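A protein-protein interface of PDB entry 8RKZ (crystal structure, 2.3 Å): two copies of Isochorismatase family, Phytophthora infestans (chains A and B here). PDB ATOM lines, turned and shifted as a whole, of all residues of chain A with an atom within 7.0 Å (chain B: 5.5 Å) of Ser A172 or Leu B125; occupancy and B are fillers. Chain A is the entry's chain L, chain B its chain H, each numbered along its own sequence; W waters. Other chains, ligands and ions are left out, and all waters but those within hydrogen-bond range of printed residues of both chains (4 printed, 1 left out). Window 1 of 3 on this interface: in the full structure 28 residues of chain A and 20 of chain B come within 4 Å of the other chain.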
ATOM      1  N   LEU A  10      -0.738  23.794  17.374  1.00  0.00           N
ATOM      2  CA  LEU A  10      -0.852  22.413  17.818  1.00  0.00           C
ATOM      3  C   LEU A  10       0.128  21.483  17.121  1.00  0.00           C
ATOM      4  O   LEU A  10       0.665  20.571  17.755  1.00  0.00           O
ATOM      5  CB  LEU A  10      -2.280  21.911  17.594  1.00  0.00           C
ATOM      6  CG  LEU A  10      -3.374  22.657  18.365  1.00  0.00           C
ATOM      7  CD1 LEU A  10      -4.592  21.775  18.502  1.00  0.00           C
ATOM      8  CD2 LEU A  10      -2.894  23.117  19.740  1.00  0.00           C
ATOM      9  N   HIS A  12      -0.611  19.292  14.731  1.00  0.00           N
ATOM     10  CA  HIS A  12      -1.200  18.006  14.394  1.00  0.00           C
ATOM     11  C   HIS A  12      -0.672  17.534  13.042  1.00  0.00           C
ATOM     12  O   HIS A  12      -0.339  18.336  12.165  1.00  0.00           O
ATOM     13  CB  HIS A  12      -2.725  18.114  14.352  1.00  0.00           C
ATOM     14  CG  HIS A  12      -3.389  17.896  15.676  1.00  0.00           C
ATOM     15  ND1 HIS A  12      -4.261  18.809  16.230  1.00  0.00           N
ATOM     16  CD2 HIS A  12      -3.316  16.867  16.553  1.00  0.00           C
ATOM     17  CE1 HIS A  12      -4.697  18.353  17.390  1.00  0.00           C
ATOM     18  NE2 HIS A  12      -4.137  17.177  17.611  1.00  0.00           N
ATOM     19  N   LEU A  13      -0.584  16.219  12.877  1.00  0.00           N
ATOM     20  CA  LEU A  13      -0.071  15.627  11.649  1.00  0.00           C
ATOM     21  C   LEU A  13      -1.124  14.696  11.068  1.00  0.00           C
ATOM     22  O   LEU A  13      -1.506  13.710  11.706  1.00  0.00           O
ATOM     23  CB  LEU A  13       1.238  14.879  11.904  1.00  0.00           C
ATOM     24  CG  LEU A  13       2.498  15.749  11.926  1.00  0.00           C
ATOM     25  CD1 LEU A  13       3.719  14.926  12.312  1.00  0.00           C
ATOM     26  CD2 LEU A  13       2.712  16.421  10.583  1.00  0.00           C
ATOM     27  N   ASP A 143      15.826  13.864  15.582  1.00  0.00           N
ATOM     28  CA  ASP A 143      16.816  12.798  15.472  1.00  0.00           C
ATOM     29  C   ASP A 143      17.115  12.414  14.026  1.00  0.00           C
ATOM     30  O   ASP A 143      17.757  11.380  13.796  1.00  0.00           O
ATOM     31  CB  ASP A 143      16.387  11.549  16.259  1.00  0.00           C
ATOM     32  CG  ASP A 143      14.915  11.212  16.097  1.00  0.00           C
ATOM     33  OD1 ASP A 143      14.184  11.972  15.425  1.00  0.00           O
ATOM     34  OD2 ASP A 143      14.499  10.154  16.621  1.00  0.00           O
ATOM     35  N   ILE A 167       9.371  20.822  16.961  1.00  0.00           N
ATOM     36  CA  ILE A 167      10.512  19.924  17.097  1.00  0.00           C
ATOM     37  C   ILE A 167       9.990  18.574  17.572  1.00  0.00           C
ATOM     38  O   ILE A 167       9.607  18.416  18.737  1.00  0.00           O
ATOM     39  CB  ILE A 167      11.567  20.487  18.056  1.00  0.00           C
ATOM     40  CG1 ILE A 167      11.915  21.927  17.667  1.00  0.00           C
ATOM     41  CG2 ILE A 167      12.808  19.615  18.031  1.00  0.00           C
ATOM     42  CD1 ILE A 167      12.408  22.083  16.244  1.00  0.00           C
ATOM     43  N   THR A 168       9.984  17.601  16.667  1.00  0.00           N
ATOM     44  CA  THR A 168       9.493  16.256  16.926  1.00  0.00           C
ATOM     45  C   THR A 168      10.635  15.259  16.741  1.00  0.00           C
ATOM     46  O   THR A 168      11.811  15.630  16.658  1.00  0.00           O
ATOM     47  CB  THR A 168       8.295  15.920  16.026  1.00  0.00           C
ATOM     48  OG1 THR A 168       7.800  14.614  16.357  1.00  0.00           O
ATOM     49  CG2 THR A 168       8.675  15.957  14.539  1.00  0.00           C
ATOM     50  N   SER A 169      10.279  13.976  16.723  1.00  0.00           N
ATOM     51  CA  SER A 169      11.230  12.896  16.510  1.00  0.00           C
ATOM     52  C   SER A 169      10.599  11.872  15.578  1.00  0.00           C
ATOM     53  O   SER A 169       9.425  11.977  15.207  1.00  0.00           O
ATOM     54  CB  SER A 169      11.646  12.253  17.836  1.00  0.00           C
ATOM     55  OG  SER A 169      10.599  11.452  18.348  1.00  0.00           O
ATOM     56  N   VAL A 170      11.389  10.862  15.207  1.00  0.00           N
ATOM     57  CA  VAL A 170      10.910   9.834  14.283  1.00  0.00           C
ATOM     58  C   VAL A 170       9.694   9.121  14.861  1.00  0.00           C
ATOM     59  O   VAL A 170       8.661   8.982  14.194  1.00  0.00           O
ATOM     60  CB  VAL A 170      12.035   8.836  13.957  1.00  0.00           C
ATOM     61  CG1 VAL A 170      11.474   7.640  13.207  1.00  0.00           C
ATOM     62  CG2 VAL A 170      13.137   9.506  13.162  1.00  0.00           C
ATOM     63  N   GLU A 171       9.793   8.659  16.112  1.00  0.00           N
ATOM     64  CA  GLU A 171       8.684   7.914  16.701  1.00  0.00           C
ATOM     65  C   GLU A 171       7.470   8.807  16.909  1.00  0.00           C
ATOM     66  O   GLU A 171       6.342   8.427  16.575  1.00  0.00           O
ATOM     67  CB  GLU A 171       9.102   7.292  18.030  1.00  0.00           C
ATOM     68  CG  GLU A 171      10.076   6.149  17.935  1.00  0.00           C
ATOM     69  CD  GLU A 171      10.147   5.385  19.237  1.00  0.00           C
ATOM     70  OE1 GLU A 171       9.154   5.419  20.006  1.00  0.00           O
ATOM     71  OE2 GLU A 171      11.205   4.786  19.513  1.00  0.00           O
ATOM     72  N   SER A 172       7.686   9.999  17.468  1.00  0.00           N
ATOM     73  CA  SER A 172       6.572  10.869  17.813  1.00  0.00           C
ATOM     74  C   SER A 172       5.799  11.298  16.571  1.00  0.00           C
ATOM     75  O   SER A 172       4.562  11.317  16.576  1.00  0.00           O
ATOM     76  CB  SER A 172       7.092  12.080  18.584  1.00  0.00           C
ATOM     77  OG  SER A 172       6.031  12.808  19.169  1.00  0.00           O
ATOM     78  N   ALA A 173       6.511  11.636  15.493  1.00  0.00           N
ATOM     79  CA  ALA A 173       5.847  12.066  14.265  1.00  0.00           C
ATOM     80  C   ALA A 173       5.132  10.909  13.573  1.00  0.00           C
ATOM     81  O   ALA A 173       4.013  11.074  13.074  1.00  0.00           O
ATOM     82  CB  ALA A 173       6.860  12.711  13.318  1.00  0.00           C
ATOM     83  N   ILE A 174       5.764   9.733  13.523  1.00  0.00           N
ATOM     84  CA  ILE A 174       5.128   8.590  12.875  1.00  0.00           C
ATOM     85  C   ILE A 174       3.865   8.189  13.628  1.00  0.00           C
ATOM     86  O   ILE A 174       2.810   7.968  13.022  1.00  0.00           O
ATOM     87  CB  ILE A 174       6.115   7.416  12.752  1.00  0.00           C
ATOM     88  CG1 ILE A 174       7.021   7.611  11.536  1.00  0.00           C
ATOM     89  CG2 ILE A 174       5.373   6.099  12.614  1.00  0.00           C
ATOM     90  CD1 ILE A 174       8.253   6.742  11.557  1.00  0.00           C
ATOM     91  N   PHE A 175       3.944   8.110  14.963  1.00  0.00           N
ATOM     92  CA  PHE A 175       2.759   7.758  15.742  1.00  0.00           C
ATOM     93  C   PHE A 175       1.678   8.824  15.629  1.00  0.00           C
ATOM     94  O   PHE A 175       0.484   8.506  15.696  1.00  0.00           O
ATOM     95  CB  PHE A 175       3.125   7.527  17.210  1.00  0.00           C
ATOM     96  CG  PHE A 175       3.580   6.125  17.503  1.00  0.00           C
ATOM     97  CD1 PHE A 175       2.665   5.088  17.586  1.00  0.00           C
ATOM     98  CD2 PHE A 175       4.923   5.846  17.703  1.00  0.00           C
ATOM     99  CE1 PHE A 175       3.083   3.796  17.851  1.00  0.00           C
ATOM    100  CE2 PHE A 175       5.350   4.554  17.974  1.00  0.00           C
ATOM    101  CZ  PHE A 175       4.430   3.529  18.046  1.00  0.00           C
ATOM    102  N   GLN A 176       2.073  10.088  15.454  1.00  0.00           N
ATOM    103  CA  GLN A 176       1.093  11.139  15.198  1.00  0.00           C
ATOM    104  C   GLN A 176       0.334  10.875  13.908  1.00  0.00           C
ATOM    105  O   GLN A 176      -0.897  10.990  13.867  1.00  0.00           O
ATOM    106  CB  GLN A 176       1.785  12.499  15.127  1.00  0.00           C
ATOM    107  CG  GLN A 176       1.844  13.262  16.432  1.00  0.00           C
ATOM    108  CD  GLN A 176       2.372  14.667  16.237  1.00  0.00           C
ATOM    109  OE1 GLN A 176       3.579  14.887  16.239  1.00  0.00           O
ATOM    110  NE2 GLN A 176       1.468  15.625  16.055  1.00  0.00           N
ATOM    111  N   LEU A 177       1.052  10.510  12.843  1.00  0.00           N
ATOM    112  CA  LEU A 177       0.391  10.221  11.576  1.00  0.00           C
ATOM    113  C   LEU A 177      -0.525   9.006  11.687  1.00  0.00           C
ATOM    114  O   LEU A 177      -1.617   8.994  11.106  1.00  0.00           O
ATOM    115  CB  LEU A 177       1.433  10.020  10.478  1.00  0.00           C
ATOM    116  CG  LEU A 177       2.208  11.285  10.099  1.00  0.00           C
ATOM    117  CD1 LEU A 177       3.556  10.948   9.482  1.00  0.00           C
ATOM    118  CD2 LEU A 177       1.378  12.148   9.155  1.00  0.00           C
ATOM    119  N   ILE A 193       8.546   0.412  13.171  1.00  0.00           N
ATOM    120  CA  ILE A 193       9.052   0.967  14.424  1.00  0.00           C
ATOM    121  C   ILE A 193       9.914  -0.060  15.142  1.00  0.00           C
ATOM    122  O   ILE A 193      10.983   0.266  15.673  1.00  0.00           O
ATOM    123  CB  ILE A 193       7.896   1.456  15.315  1.00  0.00           C
ATOM    124  CG1 ILE A 193       7.098   2.558  14.614  1.00  0.00           C
ATOM    125  CG2 ILE A 193       8.436   1.974  16.655  1.00  0.00           C
ATOM    126  CD1 ILE A 193       7.894   3.823  14.348  1.00  0.00           C
ATOM    127  N   GLU B 119       3.423   6.778  26.832  1.00  0.00           N
ATOM    128  CA  GLU B 119       4.741   7.397  26.687  1.00  0.00           C
ATOM    129  C   GLU B 119       4.593   8.895  26.440  1.00  0.00           C
ATOM    130  O   GLU B 119       3.594   9.329  25.864  1.00  0.00           O
ATOM    131  CB  GLU B 119       5.537   6.745  25.544  1.00  0.00           C
ATOM    132  CG  GLU B 119       5.847   5.266  25.751  1.00  0.00           C
ATOM    133  CD  GLU B 119       6.691   4.670  24.633  1.00  0.00           C
ATOM    134  OE1 GLU B 119       7.907   4.951  24.589  1.00  0.00           O
ATOM    135  OE2 GLU B 119       6.144   3.917  23.801  1.00  0.00           O
ATOM    136  N   THR B 120       5.598   9.675  26.857  1.00  0.00           N
ATOM    137  CA  THR B 120       5.527  11.124  26.692  1.00  0.00           C
ATOM    138  C   THR B 120       5.244  11.509  25.250  1.00  0.00           C
ATOM    139  O   THR B 120       4.385  12.358  24.984  1.00  0.00           O
ATOM    140  CB  THR B 120       6.831  11.787  27.139  1.00  0.00           C
ATOM    141  OG1 THR B 120       7.611  10.868  27.906  1.00  0.00           O
ATOM    142  CG2 THR B 120       6.544  13.026  27.960  1.00  0.00           C
ATOM    143  N   HIS B 121       5.953  10.891  24.306  1.00  0.00           N
ATOM    144  CA  HIS B 121       5.966  11.351  22.926  1.00  0.00           C
ATOM    145  C   HIS B 121       4.886  10.713  22.067  1.00  0.00           C
ATOM    146  O   HIS B 121       4.718  11.123  20.912  1.00  0.00           O
ATOM    147  CB  HIS B 121       7.344  11.091  22.303  1.00  0.00           C
ATOM    148  CG  HIS B 121       7.702   9.641  22.208  1.00  0.00           C
ATOM    149  ND1 HIS B 121       7.857   8.838  23.318  1.00  0.00           N
ATOM    150  CD2 HIS B 121       7.935   8.848  21.135  1.00  0.00           C
ATOM    151  CE1 HIS B 121       8.170   7.614  22.933  1.00  0.00           C
ATOM    152  NE2 HIS B 121       8.223   7.592  21.614  1.00  0.00           N
ATOM    153  N   VAL B 122       4.146   9.737  22.589  1.00  0.00           N
ATOM    154  CA  VAL B 122       3.111   9.117  21.776  1.00  0.00           C
ATOM    155  C   VAL B 122       1.732   9.411  22.349  1.00  0.00           C
ATOM    156  O   VAL B 122       1.003  10.263  21.829  1.00  0.00           O
ATOM    157  CB  VAL B 122       3.340   7.598  21.675  1.00  0.00           C
ATOM    158  CG1 VAL B 122       2.319   6.963  20.737  1.00  0.00           C
ATOM    159  CG2 VAL B 122       4.763   7.303  21.219  1.00  0.00           C
ATOM    160  N   CYS B 123       1.398   8.798  23.480  1.00  0.00           N
ATOM    161  CA  CYS B 123       0.028   8.905  23.961  1.00  0.00           C
ATOM    162  C   CYS B 123      -0.186  10.131  24.832  1.00  0.00           C
ATOM    163  O   CYS B 123      -1.263  10.739  24.785  1.00  0.00           O
ATOM    164  CB  CYS B 123      -0.366   7.635  24.722  1.00  0.00           C
ATOM    165  SG  CYS B 123      -0.619   6.160  23.665  1.00  0.00           S
ATOM    166  N   VAL B 124       0.824  10.516  25.612  1.00  0.00           N
ATOM    167  CA  VAL B 124       0.731  11.736  26.402  1.00  0.00           C
ATOM    168  C   VAL B 124       0.637  12.953  25.492  1.00  0.00           C
ATOM    169  O   VAL B 124      -0.194  13.845  25.706  1.00  0.00           O
ATOM    170  CB  VAL B 124       1.934  11.831  27.359  1.00  0.00           C
ATOM    171  CG1 VAL B 124       1.991  13.204  28.033  1.00  0.00           C
ATOM    172  CG2 VAL B 124       1.885  10.702  28.384  1.00  0.00           C
ATOM    173  N   LEU B 125       1.483  13.006  24.461  1.00  0.00           N
ATOM    174  CA  LEU B 125       1.518  14.172  23.584  1.00  0.00           C
ATOM    175  C   LEU B 125       0.234  14.297  22.774  1.00  0.00           C
ATOM    176  O   LEU B 125      -0.326  15.392  22.646  1.00  0.00           O
ATOM    177  CB  LEU B 125       2.732  14.094  22.659  1.00  0.00           C
ATOM    178  CG  LEU B 125       2.613  14.876  21.349  1.00  0.00           C
ATOM    179  CD1 LEU B 125       2.862  16.357  21.578  1.00  0.00           C
ATOM    180  CD2 LEU B 125       3.574  14.333  20.327  1.00  0.00           C
ATOM    181  N   GLN B 126      -0.249  13.189  22.210  1.00  0.00           N
ATOM    182  CA  GLN B 126      -1.456  13.275  21.394  1.00  0.00           C
ATOM    183  C   GLN B 126      -2.671  13.621  22.239  1.00  0.00           C
ATOM    184  O   GLN B 126      -3.580  14.313  21.762  1.00  0.00           O
ATOM    185  CB  GLN B 126      -1.665  11.974  20.624  1.00  0.00           C
ATOM    186  CG  GLN B 126      -0.578  11.742  19.593  1.00  0.00           C
ATOM    187  CD  GLN B 126      -0.845  10.558  18.692  1.00  0.00           C
ATOM    188  OE1 GLN B 126      -1.988  10.278  18.324  1.00  0.00           O
ATOM    189  NE2 GLN B 126       0.216   9.847  18.336  1.00  0.00           N
ATOM    190  N   THR B 127      -2.706  13.156  23.488  1.00  0.00           N
ATOM    191  CA  THR B 127      -3.742  13.608  24.409  1.00  0.00           C
ATOM    192  C   THR B 127      -3.624  15.101  24.669  1.00  0.00           C
ATOM    193  O   THR B 127      -4.630  15.826  24.674  1.00  0.00           O
ATOM    194  CB  THR B 127      -3.648  12.864  25.737  1.00  0.00           C
ATOM    195  OG1 THR B 127      -3.761  11.452  25.523  1.00  0.00           O
ATOM    196  CG2 THR B 127      -4.760  13.343  26.638  1.00  0.00           C
ATOM    197  N   CYS B 128      -2.398  15.571  24.903  1.00  0.00           N
ATOM    198  CA  CYS B 128      -2.185  16.980  25.206  1.00  0.00           C
ATOM    199  C   CYS B 128      -2.632  17.862  24.045  1.00  0.00           C
ATOM    200  O   CYS B 128      -3.316  18.870  24.252  1.00  0.00           O
ATOM    201  CB  CYS B 128      -0.712  17.212  25.543  1.00  0.00           C
ATOM    202  SG  CYS B 128      -0.174  18.939  25.509  1.00  0.00           S
ATOM    203  N   LEU B 129      -2.279  17.480  22.814  1.00  0.00           N
ATOM    204  CA  LEU B 129      -2.647  18.286  21.654  1.00  0.00           C
ATOM    205  C   LEU B 129      -4.157  18.312  21.446  1.00  0.00           C
ATOM    206  O   LEU B 129      -4.720  19.353  21.083  1.00  0.00           O
ATOM    207  CB  LEU B 129      -1.943  17.759  20.407  1.00  0.00           C
ATOM    208  CG  LEU B 129      -0.418  17.855  20.418  1.00  0.00           C
ATOM    209  CD1 LEU B 129       0.141  17.530  19.035  1.00  0.00           C
ATOM    210  CD2 LEU B 129       0.024  19.237  20.890  1.00  0.00           C
ATOM    211  N   ASP B 130      -4.826  17.177  21.652  1.00  0.00           N
ATOM    212  CA  ASP B 130      -6.276  17.133  21.487  1.00  0.00           C
ATOM    213  C   ASP B 130      -6.983  17.953  22.561  1.00  0.00           C
ATOM    214  O   ASP B 130      -7.988  18.617  22.281  1.00  0.00           O
ATOM    215  CB  ASP B 130      -6.760  15.683  21.509  1.00  0.00           C
ATOM    216  CG  ASP B 130      -6.485  14.959  20.203  1.00  0.00           C
ATOM    217  OD1 ASP B 130      -6.152  15.633  19.204  1.00  0.00           O
ATOM    218  OD2 ASP B 130      -6.594  13.717  20.174  1.00  0.00           O
ATOM    219  N   ASN B 152      13.277  10.829  23.844  1.00  0.00           N
ATOM    220  CA  ASN B 152      11.912  11.139  23.445  1.00  0.00           C
ATOM    221  C   ASN B 152      11.096  11.747  24.578  1.00  0.00           C
ATOM    222  O   ASN B 152      10.104  12.435  24.310  1.00  0.00           O
ATOM    223  CB  ASN B 152      11.233   9.891  22.892  1.00  0.00           C
ATOM    224  CG  ASN B 152      11.454   9.740  21.406  1.00  0.00           C
ATOM    225  OD1 ASN B 152      11.538  10.736  20.685  1.00  0.00           O
ATOM    226  ND2 ASN B 152      11.560   8.505  20.936  1.00  0.00           N
ATOM    227  N   MET B 155      12.349  15.519  24.464  1.00  0.00           N
ATOM    228  CA  MET B 155      11.758  16.060  23.246  1.00  0.00           C
ATOM    229  C   MET B 155      10.275  16.336  23.444  1.00  0.00           C
ATOM    230  O   MET B 155       9.794  17.441  23.168  1.00  0.00           O
ATOM    231  CB  MET B 155      11.990  15.080  22.092  1.00  0.00           C
ATOM    232  CG  MET B 155      11.498  15.512  20.713  1.00  0.00           C
ATOM    233  SD  MET B 155       9.709  15.495  20.516  1.00  0.00           S
ATOM    234  CE  MET B 155       9.403  13.736  20.682  1.00  0.00           C
ATOM    235  N   ALA B 156       9.535  15.342  23.946  1.00  0.00           N
ATOM    236  CA  ALA B 156       8.089  15.488  24.072  1.00  0.00           C
ATOM    237  C   ALA B 156       7.718  16.593  25.050  1.00  0.00           C
ATOM    238  O   ALA B 156       6.738  17.316  24.830  1.00  0.00           O
ATOM    239  CB  ALA B 156       7.459  14.165  24.503  1.00  0.00           C
ATOM    240  N   ARG B 159       8.191  19.748  23.231  1.00  0.00           N
ATOM    241  CA  ARG B 159       7.241  19.771  22.123  1.00  0.00           C
ATOM    242  C   ARG B 159       5.840  20.125  22.609  1.00  0.00           C
ATOM    243  O   ARG B 159       5.105  20.851  21.932  1.00  0.00           O
ATOM    244  CB  ARG B 159       7.251  18.419  21.404  1.00  0.00           C
ATOM    245  CG  ARG B 159       6.120  18.227  20.409  1.00  0.00           C
ATOM    246  CD  ARG B 159       6.235  19.192  19.237  1.00  0.00           C
ATOM    247  NE  ARG B 159       5.185  18.969  18.252  1.00  0.00           N
ATOM    248  CZ  ARG B 159       3.959  19.465  18.337  1.00  0.00           C
ATOM    249  NH1 ARG B 159       3.608  20.271  19.326  1.00  0.00           N
ATOM    250  NH2 ARG B 159       3.064  19.146  17.407  1.00  0.00           N
ATOM    251  N   MET B 160       5.452  19.625  23.783  1.00  0.00           N
ATOM    252  CA  MET B 160       4.161  20.000  24.355  1.00  0.00           C
ATOM    253  C   MET B 160       4.167  21.446  24.855  1.00  0.00           C
ATOM    254  O   MET B 160       3.201  22.188  24.636  1.00  0.00           O
ATOM    255  CB  MET B 160       3.789  19.024  25.476  1.00  0.00           C
ATOM    256  CG  MET B 160       3.218  17.705  24.963  1.00  0.00           C
ATOM    257  SD  MET B 160       2.778  16.508  26.246  1.00  0.00           S
ATOM    258  CE  MET B 160       4.394  16.009  26.830  1.00  0.00           C
HETATM  259  O   HOH W   1       2.783  10.797  18.673  1.00  0.00           O
HETATM  260  O   HOH W   2       9.626   3.718  22.236  1.00  0.00           O
HETATM  261  O   HOH W   3      10.669  19.142  21.096  1.00  0.00           O
HETATM  262  O   HOH W   4      -3.273  14.156  18.565  1.00  0.00           O
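Water W3 lies within hydrogen-bond range of O of Ile A167, O of Met B155 and N of Arg B159.
Water W1 lies within hydrogen-bond range of the side-chain amide nitrogen of Gln B126, the backbone carbonyl oxygen of Ser A172, the backbone carbonyl oxygen of His B121 and the backbone NH of Gln A176.
Water W2 bridges the side-chain carboxylate of Glu A171 (2.8 Å) and the side-chain carboxylate of Glu B119 (3.2 Å).
Water W4 lies within hydrogen-bond range of the backbone carbonyl oxygen of Gln B126 (3.2 Å), a ring nitrogen (NE2) of His A12 (3.3 Å) and the side-chain carboxylate of Asp B130 (3.3 Å).
The side-chain carboxylate of Asp B130 is in hydrogen-bond range of a ring nitrogen (NE2) of His A12, 3.0 Å away.
The backbone carbonyl oxygen (O) of Phe A175 is in hydrogen-bond range of the side-chain amide nitrogen (NE2) of Gln B126.
The guanidinium group of Arg B159 sits at hydrogen-bond distance from the backbone carbonyl oxygen of Leu A10 (2.8 Å).
The backbone carbonyl oxygen (O) of His B121 is in hydrogen-bond range of the side-chain hydroxyl (OG) of Ser A172 (2.8 Å).
OD1 of Asn B152 sits at hydrogen-bond distance from OG of Ser A169, at 2.6 Å.
The backbone carbonyl oxygen (O) of Ile A167 lies close to the side-chain sulfur (SD) of Met B155, 3.4 Å away.
The side-chain amide nitrogen of Gln B126 lies close to the backbone NH of Gln A176, 3.4 Å away.
NE2 of His B121 sits at hydrogen-bond distance from OE1 of Glu A171, 2.9 Å away.
No position is printed for both chains.
Among the printed residues, merely in contact across the chains: Leu A10 with Leu B129 (3.3 Å), His A12 with Leu B129 (3.6 Å), Ile A167 with Arg B159 (3.5 Å), Thr A168 with Met B155 (3.7 Å), Ser A169 with Met B155 (3.5 Å), Glu A171 with Asn B152 (3.8 Å), Ser A172 with Leu B125 (3.1 Å), Ser A172 with Met B155 (3.5 Å), Phe A175 with Val B122 (3.6 Å) and Gln A176 with Leu B129 (3.8 Å).
Of the 17 printed residues of chain B, 9 touch a printed residue of chain A.
Hydrophobic or aromatic side chains of chain B within 4 Å of the printed part of chain A: His B121, Val B122, Leu B125, Leu B129 and Met B155.
Hydrophobic or aromatic side chains of chain A that line the printed part of chain B: Leu A10, His A12 and Phe A175.
Among the printed residues, no Asp or Glu carboxylate lies within 4 Å of a Lys or Arg side-chain nitrogen of the other chain.
N of Ser A172 sits at hydrogen-bond distance from OG of Ser A169 (3.4 Å).
The backbone NH (N) of Leu B125 is in hydrogen-bond range of the backbone carbonyl oxygen (O) of Thr B120, at 3.0 Å.
N of Ala A173 is in hydrogen-bond range of OG1 of Thr A168 (3.4 Å).
Asp A143 touches none of the printed residues of chain B.
Printed residues of chain B within 4 Å of Ser A169: Asn B152 (2.6 Å) and Met B155 (3.5 Å).
Of chain B, only His B121 (2.8 Å), Leu B125 (3.1 Å) and Met B155 (3.5 Å) come within 4 Å of Ser A172.
Printed residues of chain A within 4 Å of Gln B126: Phe A175 and Gln A176.
Printed residues of chain A within 4 Å of Arg B159: Leu A10 and Ile A167.
Met B160 touches none of the printed residues of chain A.
The nearest residue of chain B that does not touch Ser A172 is Gln B126 (4.9 Å).
The nearest printed residue of chain A that does not touch Met B155 is Ala A173 (6.3 Å).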
